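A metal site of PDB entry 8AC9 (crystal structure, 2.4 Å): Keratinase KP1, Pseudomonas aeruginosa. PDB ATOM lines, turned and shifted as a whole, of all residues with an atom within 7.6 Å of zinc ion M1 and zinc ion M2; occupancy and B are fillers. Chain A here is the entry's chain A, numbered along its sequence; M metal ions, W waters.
OD2 of Asp 343 sits close to OG of Ser 397 (2.5 Å). NH2 of Arg 396 sits at hydrogen-bond distance from OH of Tyr 440 (3.4 Å). A ring nitrogen (NE2) of His 270 lies close to the side-chain carboxylate (OE1) of Glu 314 (3.2 Å). O of His 270 is in hydrogen-bond range of ND2 of Asn 283 (3.3 Å). O of Phe 342 sits at hydrogen-bond distance from ND2 of Asn 283, at 2.9 Å. The backbone NH (N) of Met 344 sits at hydrogen-bond distance from the side-chain amide oxygen (OD1) of Asn 283 (2.7 Å). A ring nitrogen (NE2) of His 441 lies close to the side-chain hydroxyl of Tyr 440 (3.3 Å). N of Glu 314 is in hydrogen-bond range of OD2 of Asp 272 (2.9 Å).
Merely in contact with zinc ion M1: Glu 314 and Asn 283. The nearest printed residue that does not touch zinc ion M1 is Glu 315 (4.01 Å).
Residues that only touch zinc ion M2: Tyr 440 (3.9 Å). Four residues have an atom within 4 Å of zinc ion M2: Asp 282, Glu 315, Tyr 440 and His 441. The nearest printed residue that does not touch zinc ion M2 is Glu 314 (4.1 Å).
Zinc ion M1 is bound by NE2 of His 270, OD1 of Asp 282, OD1 of Asp 343, water W1 and OD2 of Asp 343.
Zinc ion M2 is bound by water W1, at 2.1 Å. OD2 of Asp 282 binds zinc ion M2 (2.1 Å). A ring nitrogen (NE2) of His 441 binds zinc ion M2 (2.2 Å). Zinc ion M2 is bound by OE2 of Glu 315 (2.2 Å). Water W2 is bound to zinc ion M2. OE1 of Glu 315 is bound to zinc ion M2. Zinc ion M2 has six donor atoms within binding distance.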
ATOM      1  N   HIS A 270      18.379  -5.173   8.960  1.00  0.00           N
ATOM      2  CA  HIS A 270      17.710  -3.881   8.801  1.00  0.00           C
ATOM      3  C   HIS A 270      18.493  -2.987   7.842  1.00  0.00           C
ATOM      4  O   HIS A 270      19.731  -2.986   7.811  1.00  0.00           O
ATOM      5  CB  HIS A 270      17.469  -3.193  10.160  1.00  0.00           C
ATOM      6  CG  HIS A 270      18.676  -2.591  10.813  1.00  0.00           C
ATOM      7  ND1 HIS A 270      19.096  -1.301  10.574  1.00  0.00           N
ATOM      8  CD2 HIS A 270      19.491  -3.068  11.786  1.00  0.00           C
ATOM      9  CE1 HIS A 270      20.150  -1.033  11.326  1.00  0.00           C
ATOM     10  NE2 HIS A 270      20.408  -2.083  12.076  1.00  0.00           N
ATOM     11  N   ASP A 272      17.727   0.446   7.297  1.00  0.00           N
ATOM     12  CA  ASP A 272      17.768   1.862   7.671  1.00  0.00           C
ATOM     13  C   ASP A 272      19.015   2.172   8.497  1.00  0.00           C
ATOM     14  O   ASP A 272      19.586   1.292   9.159  1.00  0.00           O
ATOM     15  CB  ASP A 272      16.531   2.285   8.461  1.00  0.00           C
ATOM     16  CG  ASP A 272      16.372   1.538   9.788  1.00  0.00           C
ATOM     17  OD1 ASP A 272      16.544   0.293   9.795  1.00  0.00           O
ATOM     18  OD2 ASP A 272      16.041   2.172  10.818  1.00  0.00           O
ATOM     19  N   SER A 273      19.434   3.416   8.403  1.00  0.00           N
ATOM     20  CA  SER A 273      20.468   3.987   9.238  1.00  0.00           C
ATOM     21  C   SER A 273      19.809   4.923  10.247  1.00  0.00           C
ATOM     22  O   SER A 273      18.642   5.265  10.103  1.00  0.00           O
ATOM     23  CB  SER A 273      21.468   4.774   8.388  1.00  0.00           C
ATOM     24  OG  SER A 273      20.766   5.852   7.779  1.00  0.00           O
ATOM     25  N   VAL A 274      20.582   5.379  11.235  1.00  0.00           N
ATOM     26  CA  VAL A 274      20.141   6.498  12.077  1.00  0.00           C
ATOM     27  C   VAL A 274      20.146   7.758  11.218  1.00  0.00           C
ATOM     28  O   VAL A 274      20.669   7.762  10.092  1.00  0.00           O
ATOM     29  CB  VAL A 274      21.019   6.706  13.321  1.00  0.00           C
ATOM     30  CG1 VAL A 274      20.839   5.563  14.331  1.00  0.00           C
ATOM     31  CG2 VAL A 274      22.458   6.860  12.912  1.00  0.00           C
ATOM     32  N   ASN A 281      28.388   0.425   8.380  1.00  0.00           N
ATOM     33  CA  ASN A 281      28.486  -0.769   9.232  1.00  0.00           C
ATOM     34  C   ASN A 281      27.125  -1.114   9.825  1.00  0.00           C
ATOM     35  O   ASN A 281      26.727  -2.284   9.836  1.00  0.00           O
ATOM     36  CB  ASN A 281      29.512  -0.641  10.373  1.00  0.00           C
ATOM     37  CG  ASN A 281      29.730  -2.005  11.090  1.00  0.00           C
ATOM     38  OD1 ASN A 281      29.753  -3.049  10.429  1.00  0.00           O
ATOM     39  ND2 ASN A 281      29.819  -1.994  12.438  1.00  0.00           N
ATOM     40  N   ASP A 282      26.429  -0.101  10.336  1.00  0.00           N
ATOM     41  CA  ASP A 282      25.121  -0.273  10.972  1.00  0.00           C
ATOM     42  C   ASP A 282      24.021   0.391  10.129  1.00  0.00           C
ATOM     43  O   ASP A 282      23.736   1.574  10.304  1.00  0.00           O
ATOM     44  CB  ASP A 282      25.166   0.299  12.388  1.00  0.00           C
ATOM     45  CG  ASP A 282      23.895   0.064  13.130  1.00  0.00           C
ATOM     46  OD1 ASP A 282      23.147  -0.842  12.743  1.00  0.00           O
ATOM     47  OD2 ASP A 282      23.624   0.805  14.091  1.00  0.00           O
ATOM     48  N   ASN A 283      23.367  -0.386   9.257  1.00  0.00           N
ATOM     49  CA  ASN A 283      23.640  -1.809   9.063  1.00  0.00           C
ATOM     50  C   ASN A 283      23.727  -2.125   7.580  1.00  0.00           C
ATOM     51  O   ASN A 283      23.137  -3.113   7.103  1.00  0.00           O
ATOM     52  CB  ASN A 283      22.571  -2.694   9.735  1.00  0.00           C
ATOM     53  CG  ASN A 283      22.860  -4.203   9.573  1.00  0.00           C
ATOM     54  OD1 ASN A 283      24.014  -4.637   9.658  1.00  0.00           O
ATOM     55  ND2 ASN A 283      21.813  -4.985   9.314  1.00  0.00           N
ATOM     56  N   GLY A 284      24.441  -1.304   6.848  1.00  0.00           N
ATOM     57  CA  GLY A 284      24.775  -1.678   5.483  1.00  0.00           C
ATOM     58  C   GLY A 284      25.453  -3.027   5.413  1.00  0.00           C
ATOM     59  O   GLY A 284      25.237  -3.798   4.476  1.00  0.00           O
ATOM     60  N   GLU A 314      14.349   0.125  11.955  1.00  0.00           N
ATOM     61  CA  GLU A 314      14.872  -0.573  13.116  1.00  0.00           C
ATOM     62  C   GLU A 314      15.419   0.409  14.140  1.00  0.00           C
ATOM     63  O   GLU A 314      15.331   0.169  15.344  1.00  0.00           O
ATOM     64  CB  GLU A 314      15.971  -1.544  12.703  1.00  0.00           C
ATOM     65  CG  GLU A 314      16.536  -2.349  13.864  1.00  0.00           C
ATOM     66  CD  GLU A 314      17.754  -1.732  14.475  1.00  0.00           C
ATOM     67  OE1 GLU A 314      18.228  -0.697  13.932  1.00  0.00           O
ATOM     68  OE2 GLU A 314      18.233  -2.276  15.499  1.00  0.00           O
ATOM     69  N   GLU A 315      16.035   1.475  13.671  1.00  0.00           N
ATOM     70  CA  GLU A 315      16.639   2.460  14.552  1.00  0.00           C
ATOM     71  C   GLU A 315      15.582   3.282  15.300  1.00  0.00           C
ATOM     72  O   GLU A 315      15.931   3.961  16.258  1.00  0.00           O
ATOM     73  CB  GLU A 315      17.553   3.382  13.747  1.00  0.00           C
ATOM     74  CG  GLU A 315      18.629   2.653  12.943  1.00  0.00           C
ATOM     75  CD  GLU A 315      19.760   2.118  13.822  1.00  0.00           C
ATOM     76  OE1 GLU A 315      19.557   1.989  15.037  1.00  0.00           O
ATOM     77  OE2 GLU A 315      20.847   1.838  13.301  1.00  0.00           O
ATOM     78  N   ASN A 341      19.599 -13.340  12.077  1.00  0.00           N
ATOM     79  CA  ASN A 341      19.692 -11.883  12.077  1.00  0.00           C
ATOM     80  C   ASN A 341      21.126 -11.444  11.853  1.00  0.00           C
ATOM     81  O   ASN A 341      22.050 -11.980  12.487  1.00  0.00           O
ATOM     82  CB  ASN A 341      19.154 -11.310  13.390  1.00  0.00           C
ATOM     83  CG  ASN A 341      18.948  -9.841  13.309  1.00  0.00           C
ATOM     84  OD1 ASN A 341      18.157  -9.355  12.508  1.00  0.00           O
ATOM     85  ND2 ASN A 341      19.675  -9.103  14.134  1.00  0.00           N
ATOM     86  N   PHE A 342      21.330 -10.479  10.968  1.00  0.00           N
ATOM     87  CA  PHE A 342      22.672  -9.975  10.686  1.00  0.00           C
ATOM     88  C   PHE A 342      22.671  -8.456  10.796  1.00  0.00           C
ATOM     89  O   PHE A 342      22.264  -7.747   9.864  1.00  0.00           O
ATOM     90  CB  PHE A 342      23.144 -10.467   9.328  1.00  0.00           C
ATOM     91  CG  PHE A 342      23.105 -11.948   9.211  1.00  0.00           C
ATOM     92  CD1 PHE A 342      24.077 -12.715   9.840  1.00  0.00           C
ATOM     93  CD2 PHE A 342      22.042 -12.579   8.591  1.00  0.00           C
ATOM     94  CE1 PHE A 342      24.017 -14.090   9.802  1.00  0.00           C
ATOM     95  CE2 PHE A 342      21.974 -13.936   8.547  1.00  0.00           C
ATOM     96  CZ  PHE A 342      22.963 -14.704   9.149  1.00  0.00           C
ATOM     97  N   ASP A 343      23.151  -7.960  11.930  1.00  0.00           N
ATOM     98  CA  ASP A 343      23.115  -6.536  12.260  1.00  0.00           C
ATOM     99  C   ASP A 343      24.485  -6.126  12.794  1.00  0.00           C
ATOM    100  O   ASP A 343      24.818  -6.422  13.941  1.00  0.00           O
ATOM    101  CB  ASP A 343      22.000  -6.248  13.278  1.00  0.00           C
ATOM    102  CG  ASP A 343      21.795  -4.754  13.528  1.00  0.00           C
ATOM    103  OD1 ASP A 343      22.615  -3.932  13.045  1.00  0.00           O
ATOM    104  OD2 ASP A 343      20.792  -4.398  14.204  1.00  0.00           O
ATOM    105  N   MET A 344      25.258  -5.434  11.966  1.00  0.00           N
ATOM    106  CA  MET A 344      26.610  -4.993  12.299  1.00  0.00           C
ATOM    107  C   MET A 344      27.570  -6.176  12.281  1.00  0.00           C
ATOM    108  O   MET A 344      27.716  -6.886  13.292  1.00  0.00           O
ATOM    109  CB  MET A 344      26.648  -4.251  13.648  1.00  0.00           C
ATOM    110  CG  MET A 344      25.724  -3.012  13.758  1.00  0.00           C
ATOM    111  SD  MET A 344      26.022  -2.031  15.275  1.00  0.00           S
ATOM    112  CE  MET A 344      27.738  -1.540  15.031  1.00  0.00           C
ATOM    113  N   ARG A 396      18.119  -5.720  21.078  1.00  0.00           N
ATOM    114  CA  ARG A 396      18.420  -4.459  20.413  1.00  0.00           C
ATOM    115  C   ARG A 396      18.441  -4.588  18.896  1.00  0.00           C
ATOM    116  O   ARG A 396      18.978  -3.704  18.221  1.00  0.00           O
ATOM    117  CB  ARG A 396      19.751  -3.872  20.912  1.00  0.00           C
ATOM    118  CG  ARG A 396      19.596  -2.917  22.093  1.00  0.00           C
ATOM    119  CD  ARG A 396      20.922  -2.662  22.814  1.00  0.00           C
ATOM    120  NE  ARG A 396      21.785  -1.746  22.061  1.00  0.00           N
ATOM    121  CZ  ARG A 396      23.042  -1.474  22.392  1.00  0.00           C
ATOM    122  NH1 ARG A 396      23.586  -2.030  23.467  1.00  0.00           N
ATOM    123  NH2 ARG A 396      23.757  -0.631  21.656  1.00  0.00           N
ATOM    124  N   SER A 397      17.840  -5.647  18.357  1.00  0.00           N
ATOM    125  CA  SER A 397      17.726  -5.779  16.911  1.00  0.00           C
ATOM    126  C   SER A 397      16.477  -6.584  16.582  1.00  0.00           C
ATOM    127  O   SER A 397      15.679  -6.928  17.460  1.00  0.00           O
ATOM    128  CB  SER A 397      18.982  -6.440  16.320  1.00  0.00           C
ATOM    129  OG  SER A 397      19.137  -6.097  14.945  1.00  0.00           O
ATOM    130  N   ASP A 398      16.343  -6.958  15.304  1.00  0.00           N
ATOM    131  CA  ASP A 398      15.086  -7.347  14.712  1.00  0.00           C
ATOM    132  C   ASP A 398      14.674  -8.785  15.014  1.00  0.00           C
ATOM    133  O   ASP A 398      13.571  -9.193  14.645  1.00  0.00           O
ATOM    134  CB  ASP A 398      15.160  -7.115  13.211  1.00  0.00           C
ATOM    135  CG  ASP A 398      15.218  -5.633  12.870  1.00  0.00           C
ATOM    136  OD1 ASP A 398      14.229  -4.923  13.132  1.00  0.00           O
ATOM    137  OD2 ASP A 398      16.261  -5.183  12.373  1.00  0.00           O
ATOM    138  N   PHE A 413      27.302 -10.719  15.152  1.00  0.00           N
ATOM    139  CA  PHE A 413      27.466  -9.355  15.620  1.00  0.00           C
ATOM    140  C   PHE A 413      28.965  -9.134  15.804  1.00  0.00           C
ATOM    141  O   PHE A 413      29.645 -10.024  16.318  1.00  0.00           O
ATOM    142  CB  PHE A 413      26.682  -9.169  16.925  1.00  0.00           C
ATOM    143  CG  PHE A 413      26.781  -7.795  17.553  1.00  0.00           C
ATOM    144  CD1 PHE A 413      26.660  -6.653  16.790  1.00  0.00           C
ATOM    145  CD2 PHE A 413      26.963  -7.664  18.934  1.00  0.00           C
ATOM    146  CE1 PHE A 413      26.726  -5.383  17.388  1.00  0.00           C
ATOM    147  CE2 PHE A 413      27.026  -6.414  19.545  1.00  0.00           C
ATOM    148  CZ  PHE A 413      26.896  -5.276  18.781  1.00  0.00           C
ATOM    149  N   ALA A 416      29.352  -3.035  19.007  1.00  0.00           N
ATOM    150  CA  ALA A 416      28.974  -1.652  18.792  1.00  0.00           C
ATOM    151  C   ALA A 416      29.737  -0.734  19.739  1.00  0.00           C
ATOM    152  O   ALA A 416      30.961  -0.580  19.600  1.00  0.00           O
ATOM    153  CB  ALA A 416      27.473  -1.483  18.941  1.00  0.00           C
ATOM    154  N   TYR A 440      29.907   4.143  15.828  1.00  0.00           N
ATOM    155  CA  TYR A 440      28.540   3.732  16.043  1.00  0.00           C
ATOM    156  C   TYR A 440      27.570   4.917  15.974  1.00  0.00           C
ATOM    157  O   TYR A 440      27.713   5.905  16.690  1.00  0.00           O
ATOM    158  CB  TYR A 440      28.472   3.037  17.406  1.00  0.00           C
ATOM    159  CG  TYR A 440      27.126   2.518  17.753  1.00  0.00           C
ATOM    160  CD1 TYR A 440      26.465   1.611  16.915  1.00  0.00           C
ATOM    161  CD2 TYR A 440      26.490   2.930  18.914  1.00  0.00           C
ATOM    162  CE1 TYR A 440      25.200   1.119  17.236  1.00  0.00           C
ATOM    163  CE2 TYR A 440      25.216   2.451  19.252  1.00  0.00           C
ATOM    164  CZ  TYR A 440      24.587   1.547  18.411  1.00  0.00           C
ATOM    165  OH  TYR A 440      23.338   1.071  18.723  1.00  0.00           O
ATOM    166  N   HIS A 441      26.578   4.817  15.089  1.00  0.00           N
ATOM    167  CA  HIS A 441      25.497   5.800  15.009  1.00  0.00           C
ATOM    168  C   HIS A 441      26.029   7.195  14.727  1.00  0.00           C
ATOM    169  O   HIS A 441      25.439   8.184  15.155  1.00  0.00           O
ATOM    170  CB  HIS A 441      24.649   5.787  16.283  1.00  0.00           C
ATOM    171  CG  HIS A 441      23.673   4.648  16.346  1.00  0.00           C
ATOM    172  ND1 HIS A 441      22.653   4.572  17.271  1.00  0.00           N
ATOM    173  CD2 HIS A 441      23.558   3.530  15.578  1.00  0.00           C
ATOM    174  CE1 HIS A 441      21.954   3.464  17.073  1.00  0.00           C
ATOM    175  NE2 HIS A 441      22.482   2.817  16.046  1.00  0.00           N
ATOM    176  N   ASP A 445      30.260   6.632  10.206  1.00  0.00           N
ATOM    177  CA  ASP A 445      29.980   5.208   9.930  1.00  0.00           C
ATOM    178  C   ASP A 445      29.809   5.030   8.424  1.00  0.00           C
ATOM    179  O   ASP A 445      28.731   4.733   7.903  1.00  0.00           O
ATOM    180  CB  ASP A 445      28.747   4.710  10.692  1.00  0.00           C
ATOM    181  CG  ASP A 445      28.431   3.225  10.418  1.00  0.00           C
ATOM    182  OD1 ASP A 445      29.305   2.533   9.838  1.00  0.00           O
ATOM    183  OD2 ASP A 445      27.308   2.759  10.761  1.00  0.00           O
HETATM  184 ZN    ZN M   1      21.730  -2.058  13.589  1.00  0.00          ZN
HETATM  185 ZN    ZN M   2      21.749   0.958  15.114  1.00  0.00          ZN
HETATM  186  O   HOH W   1      20.496  -0.752  14.963  1.00  0.00           O
HETATM  187  O   HOH W   2      21.744  -0.328  17.083  1.00  0.00           O
